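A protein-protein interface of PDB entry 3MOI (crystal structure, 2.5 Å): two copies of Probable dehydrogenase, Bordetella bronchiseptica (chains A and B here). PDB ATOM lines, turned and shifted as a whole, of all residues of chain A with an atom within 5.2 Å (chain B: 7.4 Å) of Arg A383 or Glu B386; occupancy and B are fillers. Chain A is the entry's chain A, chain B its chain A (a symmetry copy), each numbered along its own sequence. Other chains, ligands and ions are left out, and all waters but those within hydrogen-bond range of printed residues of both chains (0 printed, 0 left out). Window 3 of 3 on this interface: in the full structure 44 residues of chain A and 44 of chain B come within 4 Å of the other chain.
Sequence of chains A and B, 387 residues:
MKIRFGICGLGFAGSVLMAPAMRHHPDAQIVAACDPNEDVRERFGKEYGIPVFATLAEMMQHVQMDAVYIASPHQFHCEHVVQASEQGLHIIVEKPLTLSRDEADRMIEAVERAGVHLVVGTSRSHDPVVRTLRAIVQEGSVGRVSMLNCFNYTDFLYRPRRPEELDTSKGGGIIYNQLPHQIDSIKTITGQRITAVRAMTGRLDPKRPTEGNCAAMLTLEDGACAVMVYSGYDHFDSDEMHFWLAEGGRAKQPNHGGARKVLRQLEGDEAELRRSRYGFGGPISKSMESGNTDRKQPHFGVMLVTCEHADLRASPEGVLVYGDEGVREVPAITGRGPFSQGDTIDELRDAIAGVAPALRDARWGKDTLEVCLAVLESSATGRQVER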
ATOM      1  N   VAL A 197     -11.865 -32.375  -7.000  1.00  0.00           N
ATOM      2  CA  VAL A 197     -12.178 -32.652  -8.394  1.00  0.00           C
ATOM      3  C   VAL A 197     -13.194 -31.645  -8.879  1.00  0.00           C
ATOM      4  O   VAL A 197     -14.322 -31.588  -8.333  1.00  0.00           O
ATOM      5  CB  VAL A 197     -12.831 -34.005  -8.572  1.00  0.00           C
ATOM      6  CG1 VAL A 197     -13.100 -34.238 -10.036  1.00  0.00           C
ATOM      7  CG2 VAL A 197     -11.995 -35.096  -7.978  1.00  0.00           C
ATOM      8  N   ARG A 198     -12.797 -30.874  -9.897  1.00  0.00           N
ATOM      9  CA  ARG A 198     -13.717 -30.119 -10.697  1.00  0.00           C
ATOM     10  C   ARG A 198     -13.708 -30.701 -12.110  1.00  0.00           C
ATOM     11  O   ARG A 198     -12.654 -30.669 -12.778  1.00  0.00           O
ATOM     12  CB  ARG A 198     -13.282 -28.651 -10.737  1.00  0.00           C
ATOM     13  CG  ARG A 198     -14.130 -27.762 -11.619  1.00  0.00           C
ATOM     14  CD  ARG A 198     -15.612 -27.734 -11.177  1.00  0.00           C
ATOM     15  NE  ARG A 198     -16.396 -26.915 -12.088  1.00  0.00           N
ATOM     16  CZ  ARG A 198     -17.289 -27.386 -12.945  1.00  0.00           C
ATOM     17  NH1 ARG A 198     -17.550 -28.677 -12.942  1.00  0.00           N
ATOM     18  NH2 ARG A 198     -17.937 -26.550 -13.782  1.00  0.00           N
ATOM     19  N   SER A 378     -19.222 -33.824  -9.975  1.00  0.00           N
ATOM     20  CA  SER A 378     -18.825 -32.443 -10.228  1.00  0.00           C
ATOM     21  C   SER A 378     -19.479 -31.958 -11.513  1.00  0.00           C
ATOM     22  O   SER A 378     -19.874 -30.817 -11.620  1.00  0.00           O
ATOM     23  CB  SER A 378     -17.329 -32.322 -10.399  1.00  0.00           C
ATOM     24  OG  SER A 378     -16.988 -31.000 -10.637  1.00  0.00           O
ATOM     25  N   THR A 381     -23.229 -31.176 -10.921  1.00  0.00           N
ATOM     26  CA  THR A 381     -23.551 -30.064 -10.029  1.00  0.00           C
ATOM     27  C   THR A 381     -22.857 -28.753 -10.410  1.00  0.00           C
ATOM     28  O   THR A 381     -23.234 -27.716  -9.934  1.00  0.00           O
ATOM     29  CB  THR A 381     -23.112 -30.402  -8.596  1.00  0.00           C
ATOM     30  OG1 THR A 381     -21.662 -30.511  -8.540  1.00  0.00           O
ATOM     31  CG2 THR A 381     -23.787 -31.702  -8.071  1.00  0.00           C
ATOM     32  N   GLY A 382     -21.806 -28.789 -11.239  1.00  0.00           N
ATOM     33  CA  GLY A 382     -21.009 -27.582 -11.500  1.00  0.00           C
ATOM     34  C   GLY A 382     -20.014 -27.196 -10.410  1.00  0.00           C
ATOM     35  O   GLY A 382     -19.343 -26.183 -10.538  1.00  0.00           O
ATOM     36  N   ARG A 383     -19.855 -28.002  -9.360  1.00  0.00           N
ATOM     37  CA  ARG A 383     -19.090 -27.552  -8.183  1.00  0.00           C
ATOM     38  C   ARG A 383     -17.814 -28.401  -8.092  1.00  0.00           C
ATOM     39  O   ARG A 383     -17.777 -29.547  -8.515  1.00  0.00           O
ATOM     40  CB  ARG A 383     -19.935 -27.691  -6.888  1.00  0.00           C
ATOM     41  CG  ARG A 383     -21.178 -26.646  -6.574  1.00  0.00           C
ATOM     42  CD  ARG A 383     -20.783 -25.529  -5.493  1.00  0.00           C
ATOM     43  NE  ARG A 383     -19.316 -25.765  -5.365  1.00  0.00           N
ATOM     44  CZ  ARG A 383     -18.278 -25.071  -5.891  1.00  0.00           C
ATOM     45  NH1 ARG A 383     -18.377 -23.840  -6.500  1.00  0.00           N
ATOM     46  NH2 ARG A 383     -17.118 -25.623  -5.709  1.00  0.00           N
ATOM     47  N   GLN A 384     -16.736 -27.815  -7.590  1.00  0.00           N
ATOM     48  CA  GLN A 384     -15.591 -28.588  -7.152  1.00  0.00           C
ATOM     49  C   GLN A 384     -16.013 -29.482  -6.011  1.00  0.00           C
ATOM     50  O   GLN A 384     -16.676 -29.057  -5.101  1.00  0.00           O
ATOM     51  CB  GLN A 384     -14.483 -27.698  -6.677  1.00  0.00           C
ATOM     52  CG  GLN A 384     -13.273 -28.477  -6.093  1.00  0.00           C
ATOM     53  CD  GLN A 384     -12.001 -27.656  -6.126  1.00  0.00           C
ATOM     54  OE1 GLN A 384     -11.396 -27.462  -7.171  1.00  0.00           O
ATOM     55  NE2 GLN A 384     -11.584 -27.199  -4.994  1.00  0.00           N
ATOM     56  N   VAL A 385     -15.615 -30.730  -6.078  1.00  0.00           N
ATOM     57  CA  VAL A 385     -16.016 -31.722  -5.102  1.00  0.00           C
ATOM     58  C   VAL A 385     -14.796 -32.023  -4.188  1.00  0.00           C
ATOM     59  O   VAL A 385     -13.770 -32.425  -4.651  1.00  0.00           O
ATOM     60  CB  VAL A 385     -16.538 -32.995  -5.872  1.00  0.00           C
ATOM     61  CG1 VAL A 385     -16.643 -34.186  -4.965  1.00  0.00           C
ATOM     62  CG2 VAL A 385     -17.870 -32.683  -6.576  1.00  0.00           C
ATOM     63  N   ARG B 193     -20.208 -15.662 -21.135  1.00  0.00           N
ATOM     64  CA  ARG B 193     -19.685 -15.184 -19.907  1.00  0.00           C
ATOM     65  C   ARG B 193     -18.995 -16.328 -19.146  1.00  0.00           C
ATOM     66  O   ARG B 193     -19.455 -17.475 -19.107  1.00  0.00           O
ATOM     67  CB  ARG B 193     -20.790 -14.562 -19.069  1.00  0.00           C
ATOM     68  CG  ARG B 193     -20.309 -13.996 -17.705  1.00  0.00           C
ATOM     69  CD  ARG B 193     -21.367 -13.132 -17.018  1.00  0.00           C
ATOM     70  NE  ARG B 193     -21.249 -13.175 -15.551  1.00  0.00           N
ATOM     71  CZ  ARG B 193     -20.578 -12.274 -14.837  1.00  0.00           C
ATOM     72  NH1 ARG B 193     -19.967 -11.263 -15.460  1.00  0.00           N
ATOM     73  NH2 ARG B 193     -20.490 -12.390 -13.515  1.00  0.00           N
ATOM     74  N   ILE B 194     -17.869 -15.989 -18.541  1.00  0.00           N
ATOM     75  CA  ILE B 194     -17.197 -16.868 -17.650  1.00  0.00           C
ATOM     76  C   ILE B 194     -17.872 -16.732 -16.295  1.00  0.00           C
ATOM     77  O   ILE B 194     -17.836 -15.670 -15.707  1.00  0.00           O
ATOM     78  CB  ILE B 194     -15.724 -16.457 -17.576  1.00  0.00           C
ATOM     79  CG1 ILE B 194     -15.088 -16.658 -18.954  1.00  0.00           C
ATOM     80  CG2 ILE B 194     -15.044 -17.255 -16.541  1.00  0.00           C
ATOM     81  CD1 ILE B 194     -13.708 -16.113 -19.167  1.00  0.00           C
ATOM     82  N   THR B 195     -18.467 -17.788 -15.794  1.00  0.00           N
ATOM     83  CA  THR B 195     -19.247 -17.734 -14.527  1.00  0.00           C
ATOM     84  C   THR B 195     -18.565 -18.412 -13.359  1.00  0.00           C
ATOM     85  O   THR B 195     -19.004 -18.259 -12.242  1.00  0.00           O
ATOM     86  CB  THR B 195     -20.640 -18.412 -14.639  1.00  0.00           C
ATOM     87  OG1 THR B 195     -20.453 -19.747 -15.117  1.00  0.00           O
ATOM     88  CG2 THR B 195     -21.545 -17.648 -15.626  1.00  0.00           C
ATOM     89  N   ALA B 196     -17.491 -19.151 -13.577  1.00  0.00           N
ATOM     90  CA  ALA B 196     -16.739 -19.650 -12.414  1.00  0.00           C
ATOM     91  C   ALA B 196     -15.281 -19.935 -12.800  1.00  0.00           C
ATOM     92  O   ALA B 196     -14.982 -20.192 -13.950  1.00  0.00           O
ATOM     93  CB  ALA B 196     -17.408 -20.895 -11.830  1.00  0.00           C
ATOM     94  N   VAL B 197     -14.399 -19.900 -11.815  1.00  0.00           N
ATOM     95  CA  VAL B 197     -12.962 -20.009 -12.013  1.00  0.00           C
ATOM     96  C   VAL B 197     -12.379 -20.868 -10.915  1.00  0.00           C
ATOM     97  O   VAL B 197     -12.481 -20.502  -9.720  1.00  0.00           O
ATOM     98  CB  VAL B 197     -12.268 -18.670 -11.892  1.00  0.00           C
ATOM     99  CG1 VAL B 197     -10.793 -18.851 -12.137  1.00  0.00           C
ATOM    100  CG2 VAL B 197     -12.868 -17.660 -12.821  1.00  0.00           C
ATOM    101  N   ARG B 198     -11.767 -21.984 -11.325  1.00  0.00           N
ATOM    102  CA  ARG B 198     -10.877 -22.730 -10.483  1.00  0.00           C
ATOM    103  C   ARG B 198      -9.471 -22.634 -11.073  1.00  0.00           C
ATOM    104  O   ARG B 198      -9.251 -23.102 -12.209  1.00  0.00           O
ATOM    105  CB  ARG B 198     -11.319 -24.194 -10.432  1.00  0.00           C
ATOM    106  CG  ARG B 198     -10.411 -25.105  -9.636  1.00  0.00           C
ATOM    107  CD  ARG B 198     -10.285 -24.667  -8.158  1.00  0.00           C
ATOM    108  NE  ARG B 198      -9.357 -25.536  -7.451  1.00  0.00           N
ATOM    109  CZ  ARG B 198      -8.156 -25.171  -7.031  1.00  0.00           C
ATOM    110  NH1 ARG B 198      -7.781 -23.919  -7.196  1.00  0.00           N
ATOM    111  NH2 ARG B 198      -7.347 -26.062  -6.421  1.00  0.00           N
ATOM    112  N   THR B 219     -15.413 -22.128 -15.972  1.00  0.00           N
ATOM    113  CA  THR B 219     -16.756 -22.569 -16.287  1.00  0.00           C
ATOM    114  C   THR B 219     -17.512 -21.468 -17.083  1.00  0.00           C
ATOM    115  O   THR B 219     -17.568 -20.323 -16.678  1.00  0.00           O
ATOM    116  CB  THR B 219     -17.542 -22.895 -15.035  1.00  0.00           C
ATOM    117  OG1 THR B 219     -16.853 -23.927 -14.324  1.00  0.00           O
ATOM    118  CG2 THR B 219     -18.979 -23.349 -15.404  1.00  0.00           C
ATOM    119  N   ALA B 374     -10.003 -13.442 -10.126  1.00  0.00           N
ATOM    120  CA  ALA B 374     -10.600 -14.655  -9.625  1.00  0.00           C
ATOM    121  C   ALA B 374      -9.578 -15.795  -9.696  1.00  0.00           C
ATOM    122  O   ALA B 374      -9.551 -16.687  -8.826  1.00  0.00           O
ATOM    123  CB  ALA B 374     -11.902 -14.971 -10.376  1.00  0.00           C
ATOM    124  N   GLU B 377      -7.601 -15.209  -6.535  1.00  0.00           N
ATOM    125  CA  GLU B 377      -8.321 -15.700  -5.372  1.00  0.00           C
ATOM    126  C   GLU B 377      -8.390 -17.227  -5.314  1.00  0.00           C
ATOM    127  O   GLU B 377      -8.171 -17.817  -4.239  1.00  0.00           O
ATOM    128  CB  GLU B 377      -9.721 -15.150  -5.321  1.00  0.00           C
ATOM    129  CG  GLU B 377     -10.517 -15.620  -4.101  1.00  0.00           C
ATOM    130  CD  GLU B 377     -11.956 -15.055  -4.030  1.00  0.00           C
ATOM    131  OE1 GLU B 377     -12.246 -14.020  -4.698  1.00  0.00           O
ATOM    132  OE2 GLU B 377     -12.806 -15.674  -3.306  1.00  0.00           O
ATOM    133  N   ARG B 383     -10.349 -22.921  -3.877  1.00  0.00           N
ATOM    134  CA  ARG B 383     -11.790 -23.139  -4.097  1.00  0.00           C
ATOM    135  C   ARG B 383     -12.145 -22.606  -5.493  1.00  0.00           C
ATOM    136  O   ARG B 383     -11.522 -21.687  -6.003  1.00  0.00           O
ATOM    137  CB  ARG B 383     -12.630 -22.422  -3.006  1.00  0.00           C
ATOM    138  CG  ARG B 383     -12.698 -23.016  -1.465  1.00  0.00           C
ATOM    139  CD  ARG B 383     -14.066 -23.800  -1.168  1.00  0.00           C
ATOM    140  NE  ARG B 383     -14.658 -23.864  -2.536  1.00  0.00           N
ATOM    141  CZ  ARG B 383     -14.706 -24.898  -3.410  1.00  0.00           C
ATOM    142  NH1 ARG B 383     -14.389 -26.204  -3.110  1.00  0.00           N
ATOM    143  NH2 ARG B 383     -15.167 -24.586  -4.583  1.00  0.00           N
ATOM    144  N   GLN B 384     -13.117 -23.229  -6.146  1.00  0.00           N
ATOM    145  CA  GLN B 384     -13.755 -22.630  -7.299  1.00  0.00           C
ATOM    146  C   GLN B 384     -14.442 -21.355  -6.872  1.00  0.00           C
ATOM    147  O   GLN B 384     -15.122 -21.319  -5.879  1.00  0.00           O
ATOM    148  CB  GLN B 384     -14.780 -23.549  -7.893  1.00  0.00           C
ATOM    149  CG  GLN B 384     -15.573 -22.912  -9.067  1.00  0.00           C
ATOM    150  CD  GLN B 384     -16.181 -23.961  -9.974  1.00  0.00           C
ATOM    151  OE1 GLN B 384     -15.493 -24.599 -10.759  1.00  0.00           O
ATOM    152  NE2 GLN B 384     -17.458 -24.123  -9.888  1.00  0.00           N
ATOM    153  N   VAL B 385     -14.250 -20.310  -7.640  1.00  0.00           N
ATOM    154  CA  VAL B 385     -14.773 -19.001  -7.308  1.00  0.00           C
ATOM    155  C   VAL B 385     -15.974 -18.706  -8.249  1.00  0.00           C
ATOM    156  O   VAL B 385     -15.834 -18.703  -9.435  1.00  0.00           O
ATOM    157  CB  VAL B 385     -13.607 -17.948  -7.450  1.00  0.00           C
ATOM    158  CG1 VAL B 385     -14.130 -16.542  -7.467  1.00  0.00           C
ATOM    159  CG2 VAL B 385     -12.558 -18.163  -6.344  1.00  0.00           C
ATOM    160  N   GLU B 386     -17.159 -18.484  -7.712  1.00  0.00           N
ATOM    161  CA  GLU B 386     -18.326 -18.153  -8.554  1.00  0.00           C
ATOM    162  C   GLU B 386     -18.397 -16.678  -8.864  1.00  0.00           C
ATOM    163  O   GLU B 386     -18.228 -15.882  -7.993  1.00  0.00           O
ATOM    164  CB  GLU B 386     -19.591 -18.519  -7.821  1.00  0.00           C
ATOM    165  CG  GLU B 386     -19.668 -19.971  -7.392  1.00  0.00           C
ATOM    166  CD  GLU B 386     -19.795 -20.938  -8.565  1.00  0.00           C
ATOM    167  OE1 GLU B 386     -20.241 -20.482  -9.647  1.00  0.00           O
ATOM    168  OE2 GLU B 386     -19.440 -22.150  -8.400  1.00  0.00           O
ATOM    169  N   ARG B 387     -18.727 -16.286 -10.074  1.00  0.00           N
ATOM    170  CA  ARG B 387     -18.961 -14.844 -10.273  1.00  0.00           C
ATOM    171  C   ARG B 387     -20.126 -14.404 -11.155  1.00  0.00           C
ATOM    172  O   ARG B 387     -20.795 -15.266 -11.722  1.00  0.00           O
ATOM    173  CB  ARG B 387     -17.688 -14.208 -10.745  1.00  0.00           C
ATOM    174  CG  ARG B 387     -17.143 -14.672 -12.056  1.00  0.00           C
ATOM    175  CD  ARG B 387     -16.063 -13.610 -12.474  1.00  0.00           C
ATOM    176  NE  ARG B 387     -16.211 -13.514 -13.869  1.00  0.00           N
ATOM    177  CZ  ARG B 387     -16.503 -12.472 -14.619  1.00  0.00           C
ATOM    178  NH1 ARG B 387     -16.488 -11.244 -14.213  1.00  0.00           N
ATOM    179  NH2 ARG B 387     -16.712 -12.735 -15.883  1.00  0.00           N
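Gln B384 touches Arg A383 (NE2 to NH1, 3.5 Å). NH1 of Arg B383 touches NE2 of Gln A384 (3.5 Å).
The side-chain hydroxyl of Ser A378 is in hydrogen-bond range of the guanidinium group of Arg A198, at 3.3 Å. NE of Arg A198 lies close to O of Gly A382, 3.4 Å away. The backbone carbonyl oxygen (O) of Arg A383 sits at hydrogen-bond distance from the side-chain hydroxyl (OG) of Ser A378 (2.7 Å). OG1 of Thr A381 sits at hydrogen-bond distance from N of Arg A383 (3.2 Å). N of Thr B195 lies within hydrogen-bond range of O of Thr B219, 2.8 Å away. The side-chain amide nitrogen (NE2) of Gln B384 is in hydrogen-bond range of the side-chain carboxylate (OE2) of Glu B386.
The guanidinium group (NH2) of Arg A198 is in hydrogen-bond range of the side-chain hydroxyl (OG1) of Thr B219 (2.9 Å). The side-chain amide oxygen of Gln B384 is in hydrogen-bond range of the guanidinium group of Arg A198, 2.8 Å away. The side-chain amide nitrogen of Gln B384 is in hydrogen-bond range of the backbone carbonyl oxygen of Gly A382, at 2.9 Å. The guanidinium group (NH2) of Arg B383 sits close to the guanidinium group (NH2) of Arg A383 (2.5 Å). The guanidinium group (NH1) of Arg A383 is in salt-bridge range of the side-chain carboxylate (OE2) of Glu B386 (2.8 Å). NE of Arg B198 lies within hydrogen-bond range of OE1 of Gln A384 (2.8 Å).
Arg A383 touches three residues of chain B. Printed residues of chain A within 4 Å of Gln B384: Arg A198 (2.8 Å), Gly A382 (2.9 Å) and Arg A383 (3.5 Å). Printed residues of chain B within 4 Å of Arg A198: Thr B219 (2.9 Å) and Gln B384 (2.8 Å). Printed residues of chain A within 4 Å of Arg B198: Gln A384. Of the printed residues of chain A, Thr B219 touches Arg A198. Printed residues of chain A within 4 Å of Arg B383: Arg A383 and Gln A384. Ala B374 touches none of the printed residues of chain A. The nearest residue of chain B that does not touch Arg A383 is Val B385 (5.5 Å). The nearest residue of chain A that does not touch Glu B386 is Gly A382 (4.6 Å).
Arg A198 touches Gln B384, and with the chains exchanged Gln A384 touches Arg B198. Arg B383 touches its own counterpart, Arg A383. Arg A383 touches Gln B384, and with the chains exchanged Gln A384 touches Arg B383. Positions printed for both chains: 197, 198, 383, 384 and 385.
Of the 14 printed residues of chain B, 5 touch a printed residue of chain A. Along chain B the printed residues that touch a printed residue of chain A span positions 198 to 386. Of the 8 printed residues of chain A, 4 touch a printed residue of chain B. Printed residues of chain A that touch a printed residue of chain B: Arg A198, Gly A382, Arg A383 and Gln A384. Among the printed residues, Asp or Glu carboxylates within 4 Å of a Lys or Arg side-chain nitrogen of the other chain: Arg A383 with Glu B386.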
